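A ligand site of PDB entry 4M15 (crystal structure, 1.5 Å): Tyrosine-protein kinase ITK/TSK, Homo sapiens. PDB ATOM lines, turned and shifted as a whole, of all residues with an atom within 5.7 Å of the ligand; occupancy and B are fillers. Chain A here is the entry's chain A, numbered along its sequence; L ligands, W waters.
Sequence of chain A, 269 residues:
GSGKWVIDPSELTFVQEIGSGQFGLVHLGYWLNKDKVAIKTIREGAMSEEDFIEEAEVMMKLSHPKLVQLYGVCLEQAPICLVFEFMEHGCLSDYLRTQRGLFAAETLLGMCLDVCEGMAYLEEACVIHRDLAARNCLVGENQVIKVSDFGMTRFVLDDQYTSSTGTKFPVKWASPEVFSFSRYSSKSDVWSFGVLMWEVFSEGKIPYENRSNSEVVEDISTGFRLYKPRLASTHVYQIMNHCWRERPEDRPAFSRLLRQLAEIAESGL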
ATOM      1  N   ILE A  18      -3.045  30.204   4.972  1.00  0.00           N
ATOM      2  CA  ILE A  18      -2.270  29.167   4.282  1.00  0.00           C
ATOM      3  C   ILE A  18      -2.284  29.501   2.787  1.00  0.00           C
ATOM      4  O   ILE A  18      -1.242  29.476   2.141  1.00  0.00           O
ATOM      5  CB  ILE A  18      -2.863  27.743   4.522  1.00  0.00           C
ATOM      6  CG1 ILE A  18      -2.638  27.279   5.963  1.00  0.00           C
ATOM      7  CG2 ILE A  18      -2.270  26.728   3.517  1.00  0.00           C
ATOM      8  CD1 ILE A  18      -3.203  25.924   6.272  1.00  0.00           C
ATOM      9  N   GLY A  19      -3.471  29.804   2.259  1.00  0.00           N
ATOM     10  CA  GLY A  19      -3.604  30.149   0.857  1.00  0.00           C
ATOM     11  C   GLY A  19      -5.035  30.384   0.432  1.00  0.00           C
ATOM     12  O   GLY A  19      -5.927  30.445   1.269  1.00  0.00           O
ATOM     13  N   SER A  20      -5.231  30.576  -0.882  1.00  0.00           N
ATOM     14  CA  SER A  20      -6.533  30.802  -1.491  1.00  0.00           C
ATOM     15  C   SER A  20      -6.892  29.593  -2.339  1.00  0.00           C
ATOM     16  O   SER A  20      -6.072  29.055  -3.068  1.00  0.00           O
ATOM     17  CB  SER A  20      -6.512  32.049  -2.369  1.00  0.00           C
ATOM     18  OG  SER A  20      -6.712  33.226  -1.606  1.00  0.00           O
ATOM     19  N   GLY A  21      -8.134  29.164  -2.188  1.00  0.00           N
ATOM     20  CA  GLY A  21      -8.685  28.049  -2.951  1.00  0.00           C
ATOM     21  C   GLY A  21      -9.718  28.540  -3.932  1.00  0.00           C
ATOM     22  O   GLY A  21      -9.954  29.755  -4.050  1.00  0.00           O
ATOM     23  N   GLN A  22     -10.339  27.592  -4.655  1.00  0.00           N
ATOM     24  CA  GLN A  22     -11.391  27.834  -5.641  1.00  0.00           C
ATOM     25  C   GLN A  22     -12.558  28.605  -5.024  1.00  0.00           C
ATOM     26  O   GLN A  22     -13.081  29.539  -5.635  1.00  0.00           O
ATOM     27  CB  GLN A  22     -11.905  26.468  -6.172  1.00  0.00           C
ATOM     28  CG  GLN A  22     -12.295  26.472  -7.645  1.00  0.00           C
ATOM     29  CD  GLN A  22     -12.528  25.073  -8.182  1.00  0.00           C
ATOM     30  OE1 GLN A  22     -11.730  24.153  -7.961  1.00  0.00           O
ATOM     31  NE2 GLN A  22     -13.599  24.896  -8.939  1.00  0.00           N
ATOM     32  N   PHE A  23     -12.961  28.228  -3.804  1.00  0.00           N
ATOM     33  CA  PHE A  23     -14.127  28.837  -3.160  1.00  0.00           C
ATOM     34  C   PHE A  23     -13.876  29.706  -1.935  1.00  0.00           C
ATOM     35  O   PHE A  23     -14.814  30.234  -1.339  1.00  0.00           O
ATOM     36  CB  PHE A  23     -15.225  27.778  -2.940  1.00  0.00           C
ATOM     37  CG  PHE A  23     -15.436  26.894  -4.148  1.00  0.00           C
ATOM     38  CD1 PHE A  23     -15.825  27.437  -5.367  1.00  0.00           C
ATOM     39  CD2 PHE A  23     -15.211  25.528  -4.074  1.00  0.00           C
ATOM     40  CE1 PHE A  23     -15.997  26.620  -6.498  1.00  0.00           C
ATOM     41  CE2 PHE A  23     -15.395  24.713  -5.198  1.00  0.00           C
ATOM     42  CZ  PHE A  23     -15.788  25.269  -6.396  1.00  0.00           C
ATOM     43  N   VAL A  26      -8.017  29.552   2.997  1.00  0.00           N
ATOM     44  CA  VAL A  26      -7.638  28.404   3.836  1.00  0.00           C
ATOM     45  C   VAL A  26      -6.725  28.976   4.902  1.00  0.00           C
ATOM     46  O   VAL A  26      -5.772  29.711   4.574  1.00  0.00           O
ATOM     47  CB  VAL A  26      -6.918  27.283   3.075  1.00  0.00           C
ATOM     48  CG1 VAL A  26      -6.685  26.085   4.001  1.00  0.00           C
ATOM     49  CG2 VAL A  26      -7.723  26.861   1.839  1.00  0.00           C
ATOM     50  N   ALA A  38      -6.619  22.718   9.385  1.00  0.00           N
ATOM     51  CA  ALA A  38      -6.704  23.606   8.218  1.00  0.00           C
ATOM     52  C   ALA A  38      -8.201  23.946   8.090  1.00  0.00           C
ATOM     53  O   ALA A  38      -9.053  23.048   8.047  1.00  0.00           O
ATOM     54  CB  ALA A  38      -6.233  22.881   6.975  1.00  0.00           C
ATOM     55  N   LYS A  40     -11.172  25.783   5.842  1.00  0.00           N
ATOM     56  CA  LYS A  40     -11.470  26.311   4.508  1.00  0.00           C
ATOM     57  C   LYS A  40     -12.770  27.091   4.607  1.00  0.00           C
ATOM     58  O   LYS A  40     -13.789  26.510   4.953  1.00  0.00           O
ATOM     59  CB  LYS A  40     -11.596  25.180   3.484  1.00  0.00           C
ATOM     60  CG  LYS A  40     -10.310  24.414   3.228  1.00  0.00           C
ATOM     61  CD  LYS A  40     -10.405  23.606   1.931  1.00  0.00           C
ATOM     62  CE  LYS A  40      -9.334  22.568   1.823  1.00  0.00           C
ATOM     63  NZ  LYS A  40      -9.585  21.632   0.693  1.00  0.00           N
ATOM     64  N   VAL A  68      -7.448  12.272   4.224  1.00  0.00           N
ATOM     65  CA  VAL A  68      -7.460  13.500   5.045  1.00  0.00           C
ATOM     66  C   VAL A  68      -8.812  13.545   5.767  1.00  0.00           C
ATOM     67  O   VAL A  68      -9.862  13.537   5.103  1.00  0.00           O
ATOM     68  CB  VAL A  68      -7.269  14.756   4.168  1.00  0.00           C
ATOM     69  CG1 VAL A  68      -7.395  16.038   5.002  1.00  0.00           C
ATOM     70  CG2 VAL A  68      -5.913  14.745   3.445  1.00  0.00           C
ATOM     71  N   PHE A  84     -10.472  20.663   8.559  1.00  0.00           N
ATOM     72  CA  PHE A  84      -9.760  19.463   8.135  1.00  0.00           C
ATOM     73  C   PHE A  84      -8.524  19.199   8.968  1.00  0.00           C
ATOM     74  O   PHE A  84      -7.930  20.106   9.571  1.00  0.00           O
ATOM     75  CB  PHE A  84      -9.240  19.661   6.687  1.00  0.00           C
ATOM     76  CG  PHE A  84     -10.283  19.754   5.601  1.00  0.00           C
ATOM     77  CD1 PHE A  84     -10.699  18.632   4.902  1.00  0.00           C
ATOM     78  CD2 PHE A  84     -10.806  20.999   5.226  1.00  0.00           C
ATOM     79  CE1 PHE A  84     -11.637  18.726   3.865  1.00  0.00           C
ATOM     80  CE2 PHE A  84     -11.769  21.096   4.201  1.00  0.00           C
ATOM     81  CZ  PHE A  84     -12.171  19.961   3.517  1.00  0.00           C
ATOM     82  N   GLU A  85      -8.067  17.959   8.900  1.00  0.00           N
ATOM     83  CA  GLU A  85      -6.782  17.569   9.422  1.00  0.00           C
ATOM     84  C   GLU A  85      -5.690  18.437   8.707  1.00  0.00           C
ATOM     85  O   GLU A  85      -5.747  18.599   7.486  1.00  0.00           O
ATOM     86  CB  GLU A  85      -6.611  16.093   9.009  1.00  0.00           C
ATOM     87  CG  GLU A  85      -5.304  15.456   9.358  1.00  0.00           C
ATOM     88  CD  GLU A  85      -5.142  14.036   8.850  1.00  0.00           C
ATOM     89  OE1 GLU A  85      -6.137  13.391   8.428  1.00  0.00           O
ATOM     90  OE2 GLU A  85      -4.002  13.550   8.972  1.00  0.00           O
ATOM     91  N   PHE A  86      -4.710  18.980   9.473  1.00  0.00           N
ATOM     92  CA  PHE A  86      -3.671  19.800   8.884  1.00  0.00           C
ATOM     93  C   PHE A  86      -2.588  18.933   8.239  1.00  0.00           C
ATOM     94  O   PHE A  86      -2.043  18.028   8.899  1.00  0.00           O
ATOM     95  CB  PHE A  86      -3.055  20.732   9.948  1.00  0.00           C
ATOM     96  CG  PHE A  86      -1.922  21.573   9.413  1.00  0.00           C
ATOM     97  CD1 PHE A  86      -2.159  22.585   8.481  1.00  0.00           C
ATOM     98  CD2 PHE A  86      -0.623  21.369   9.837  1.00  0.00           C
ATOM     99  CE1 PHE A  86      -1.102  23.360   7.988  1.00  0.00           C
ATOM    100  CE2 PHE A  86       0.424  22.134   9.343  1.00  0.00           C
ATOM    101  CZ  PHE A  86       0.172  23.131   8.432  1.00  0.00           C
ATOM    102  N   MET A  87      -2.298  19.222   6.959  1.00  0.00           N
ATOM    103  CA  MET A  87      -1.295  18.475   6.156  1.00  0.00           C
ATOM    104  C   MET A  87      -0.127  19.415   5.917  1.00  0.00           C
ATOM    105  O   MET A  87      -0.217  20.315   5.082  1.00  0.00           O
ATOM    106  CB  MET A  87      -1.942  17.951   4.847  1.00  0.00           C
ATOM    107  CG  MET A  87      -3.158  17.034   5.097  1.00  0.00           C
ATOM    108  SD  MET A  87      -2.739  15.529   5.981  1.00  0.00           S
ATOM    109  CE  MET A  87      -1.780  14.701   4.704  1.00  0.00           C
ATOM    110  N   GLU A  88       0.932  19.234   6.695  1.00  0.00           N
ATOM    111  CA  GLU A  88       2.075  20.157   6.724  1.00  0.00           C
ATOM    112  C   GLU A  88       2.740  20.548   5.417  1.00  0.00           C
ATOM    113  O   GLU A  88       3.214  21.670   5.290  1.00  0.00           O
ATOM    114  CB  GLU A  88       3.080  19.766   7.813  1.00  0.00           C
ATOM    115  CG  GLU A  88       3.861  18.494   7.572  1.00  0.00           C
ATOM    116  CD  GLU A  88       4.907  18.238   8.643  1.00  0.00           C
ATOM    117  OE1 GLU A  88       5.828  19.074   8.791  1.00  0.00           O
ATOM    118  OE2 GLU A  88       4.789  17.212   9.352  1.00  0.00           O
ATOM    119  N   HIS A  89       2.816  19.605   4.460  1.00  0.00           N
ATOM    120  CA  HIS A  89       3.498  19.913   3.194  1.00  0.00           C
ATOM    121  C   HIS A  89       2.593  20.319   2.032  1.00  0.00           C
ATOM    122  O   HIS A  89       3.061  20.477   0.916  1.00  0.00           O
ATOM    123  CB  HIS A  89       4.470  18.812   2.814  1.00  0.00           C
ATOM    124  CG  HIS A  89       5.591  18.660   3.786  1.00  0.00           C
ATOM    125  ND1 HIS A  89       5.661  17.589   4.641  1.00  0.00           N
ATOM    126  CD2 HIS A  89       6.621  19.493   4.039  1.00  0.00           C
ATOM    127  CE1 HIS A  89       6.756  17.774   5.363  1.00  0.00           C
ATOM    128  NE2 HIS A  89       7.362  18.903   5.037  1.00  0.00           N
ATOM    129  N   GLY A  90       1.310  20.504   2.305  1.00  0.00           N
ATOM    130  CA  GLY A  90       0.404  20.996   1.274  1.00  0.00           C
ATOM    131  C   GLY A  90       0.051  20.038   0.153  1.00  0.00           C
ATOM    132  O   GLY A  90       0.114  18.816   0.327  1.00  0.00           O
ATOM    133  N   CYS A  91      -0.413  20.581  -0.977  1.00  0.00           N
ATOM    134  CA  CYS A  91      -0.848  19.687  -2.040  1.00  0.00           C
ATOM    135  C   CYS A  91       0.253  18.966  -2.769  1.00  0.00           C
ATOM    136  O   CYS A  91       1.368  19.479  -2.923  1.00  0.00           O
ATOM    137  CB  CYS A  91      -1.854  20.333  -2.976  1.00  0.00           C
ATOM    138  SG  CYS A  91      -1.134  21.508  -4.128  1.00  0.00           S
ATOM    139  N   ASP A  94       1.922  20.614  -6.101  1.00  0.00           N
ATOM    140  CA  ASP A  94       2.947  21.630  -5.777  1.00  0.00           C
ATOM    141  C   ASP A  94       4.195  20.998  -5.155  1.00  0.00           C
ATOM    142  O   ASP A  94       5.319  21.400  -5.467  1.00  0.00           O
ATOM    143  CB  ASP A  94       2.355  22.673  -4.808  1.00  0.00           C
ATOM    144  CG  ASP A  94       1.320  23.590  -5.417  1.00  0.00           C
ATOM    145  OD1 ASP A  94       1.291  23.736  -6.657  1.00  0.00           O
ATOM    146  OD2 ASP A  94       0.546  24.199  -4.646  1.00  0.00           O
ATOM    147  N   ARG A 135      -3.658  17.297  -7.419  1.00  0.00           N
ATOM    148  CA  ARG A 135      -4.052  18.563  -6.746  1.00  0.00           C
ATOM    149  C   ARG A 135      -4.976  18.309  -5.544  1.00  0.00           C
ATOM    150  O   ARG A 135      -5.075  19.159  -4.655  1.00  0.00           O
ATOM    151  CB  ARG A 135      -4.706  19.540  -7.734  1.00  0.00           C
ATOM    152  CG  ARG A 135      -5.959  19.003  -8.394  1.00  0.00           C
ATOM    153  CD  ARG A 135      -6.446  19.831  -9.566  1.00  0.00           C
ATOM    154  NE  ARG A 135      -7.064  18.977 -10.591  1.00  0.00           N
ATOM    155  CZ  ARG A 135      -8.302  18.498 -10.529  1.00  0.00           C
ATOM    156  NH1 ARG A 135      -9.077  18.785  -9.490  1.00  0.00           N
ATOM    157  NH2 ARG A 135      -8.765  17.732 -11.493  1.00  0.00           N
ATOM    158  N   ASN A 136      -5.672  17.139  -5.526  1.00  0.00           N
ATOM    159  CA  ASN A 136      -6.569  16.768  -4.431  1.00  0.00           C
ATOM    160  C   ASN A 136      -5.957  15.809  -3.403  1.00  0.00           C
ATOM    161  O   ASN A 136      -6.678  15.234  -2.567  1.00  0.00           O
ATOM    162  CB  ASN A 136      -7.883  16.189  -4.979  1.00  0.00           C
ATOM    163  CG  ASN A 136      -8.793  17.258  -5.473  1.00  0.00           C
ATOM    164  OD1 ASN A 136      -8.833  18.352  -4.924  1.00  0.00           O
ATOM    165  ND2 ASN A 136      -9.522  16.967  -6.534  1.00  0.00           N
ATOM    166  N   LEU A 138      -2.864  15.413  -0.469  1.00  0.00           N
ATOM    167  CA  LEU A 138      -2.063  16.247   0.417  1.00  0.00           C
ATOM    168  C   LEU A 138      -0.920  15.481   1.025  1.00  0.00           C
ATOM    169  O   LEU A 138      -0.976  14.241   1.143  1.00  0.00           O
ATOM    170  CB  LEU A 138      -2.976  16.865   1.478  1.00  0.00           C
ATOM    171  CG  LEU A 138      -3.943  17.938   0.917  1.00  0.00           C
ATOM    172  CD1 LEU A 138      -5.189  18.087   1.774  1.00  0.00           C
ATOM    173  CD2 LEU A 138      -3.286  19.304   0.881  1.00  0.00           C
ATOM    174  N   ASP A 149     -11.116  15.559  -0.572  1.00  0.00           N
ATOM    175  CA  ASP A 149     -12.104  16.123  -1.482  1.00  0.00           C
ATOM    176  C   ASP A 149     -12.964  15.113  -2.251  1.00  0.00           C
ATOM    177  O   ASP A 149     -13.666  15.451  -3.202  1.00  0.00           O
ATOM    178  CB  ASP A 149     -11.464  17.168  -2.441  1.00  0.00           C
ATOM    179  CG  ASP A 149     -10.930  18.432  -1.798  1.00  0.00           C
ATOM    180  OD1 ASP A 149     -10.756  18.449  -0.550  1.00  0.00           O
ATOM    181  OD2 ASP A 149     -10.605  19.387  -2.536  1.00  0.00           O
HETATM  182  P1  LIG L   1      -8.234  24.588  -4.530  1.00  0.00           P
HETATM  183  O1  LIG L   1      -9.517  23.787  -4.175  1.00  0.00           O
HETATM  184  O2  LIG L   1      -7.168  23.584  -5.001  1.00  0.00           O
HETATM  185  O3  LIG L   1      -8.451  25.696  -5.493  1.00  0.00           O
HETATM  186  P2  LIG L   1      -7.372  23.957  -1.965  1.00  0.00           P
HETATM  187  O4  LIG L   1      -7.074  22.556  -2.304  1.00  0.00           O
HETATM  188  O5  LIG L   1      -8.548  24.251  -1.025  1.00  0.00           O
HETATM  189  O6  LIG L   1      -7.664  25.009  -3.093  1.00  0.00           O
HETATM  190  O7  LIG L   1      -6.219  24.657  -1.104  1.00  0.00           O
HETATM  191  C1  LIG L   1      -5.530  25.911  -1.268  1.00  0.00           C
HETATM  192  C2  LIG L   1      -4.274  25.866  -0.436  1.00  0.00           C
HETATM  193  O8  LIG L   1      -4.569  25.335   0.881  1.00  0.00           O
HETATM  194  C3  LIG L   1      -3.103  25.062  -0.987  1.00  0.00           C
HETATM  195  O9  LIG L   1      -1.885  25.795  -0.840  1.00  0.00           O
HETATM  196  C4  LIG L   1      -3.141  23.775  -0.164  1.00  0.00           C
HETATM  197  O10 LIG L   1      -1.848  23.209  -0.003  1.00  0.00           O
HETATM  198  C5  LIG L   1      -3.676  24.272   1.184  1.00  0.00           C
HETATM  199  N1  LIG L   1      -4.425  23.268   1.951  1.00  0.00           N
HETATM  200  C6  LIG L   1      -5.671  22.789   1.650  1.00  0.00           C
HETATM  201  N2  LIG L   1      -6.112  21.880   2.479  1.00  0.00           N
HETATM  202  C7  LIG L   1      -5.093  21.743   3.402  1.00  0.00           C
HETATM  203  C8  LIG L   1      -4.943  20.940   4.548  1.00  0.00           C
HETATM  204  N3  LIG L   1      -5.834  20.008   4.922  1.00  0.00           N
HETATM  205  N4  LIG L   1      -3.801  21.073   5.268  1.00  0.00           N
HETATM  206  C9  LIG L   1      -2.865  21.947   4.856  1.00  0.00           C
HETATM  207  N5  LIG L   1      -2.887  22.749   3.788  1.00  0.00           N
HETATM  208  C10 LIG L   1      -4.041  22.607   3.096  1.00  0.00           C
HETATM  209  O   HOH W   1      -8.077  19.622   2.844  1.00  0.00           O
HETATM  210  O   HOH W   2      -0.314  23.841   3.162  1.00  0.00           O
HETATM  211  O   HOH W   3       0.389  23.534  -1.374  1.00  0.00           O
HETATM  212  O   HOH W   4      -2.907  28.485  -2.399  1.00  0.00           O
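The side-chain sulfur of Cys 91 lies within hydrogen-bond range of the side-chain carboxylate of Asp 94, at 3.2 Å.
The side-chain carboxylate of Asp 149 is in salt-bridge range of the side-chain amino group of Lys 40.
The backbone carbonyl oxygen (O) of Ala 38 is in hydrogen-bond range of the backbone NH (N) of Phe 84 (2.8 Å).
The backbone carbonyl oxygen (O) of Val 26 sits at hydrogen-bond distance from the backbone NH (N) of Ile 18 (2.8 Å).
The backbone carbonyl oxygen (O) of Gly 19 lies within hydrogen-bond range of the backbone NH (N) of Val 26, 2.9 Å away.
The backbone NH (N) of Gln 22 lies within hydrogen-bond range of an oxygen (O3) of the ligand, 2.8 Å away.
The backbone NH (N) of Met 87 lies within hydrogen-bond range of a nitrogen (N4) of the ligand, 2.9 Å away.
The backbone carbonyl oxygen of Glu 85 lies within hydrogen-bond range of a nitrogen (N3) of the ligand (2.9 Å).
N of Cys 91 is in hydrogen-bond range of O10 of the ligand (3.1 Å).
An oxygen (O5) of the ligand lies within salt-bridge range of the side-chain amino group of Lys 40 (3.3 Å).
Merely in contact with the ligand: Gly 21 (3.2 Å), Ala 38 (3.4 Å), Gly 90 (3.4 Å), Val 26 (3.6 Å), Ser 20 (3.7 Å), Ile 18 (3.7 Å), Leu 138 (3.7 Å), Phe 86 (3.7 Å) and Phe 84 (3.9 Å).
Of the 23 residues printed, 14 come within 4 Å of the ligand.
The nearest printed residue that does not touch the ligand is Val 68 (4.3 Å).
Water W3 lies within hydrogen-bond range of an oxygen (O10) of the ligand, the backbone NH (N) of Cys 91 and the side-chain carboxylate (OD2) of Asp 94.
Water W1 bridges N2 of the ligand and NZ of Lys 40.
Water W4 bridges O9 of the ligand (3.3 Å) and O of Ser 20 (3.3 Å).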
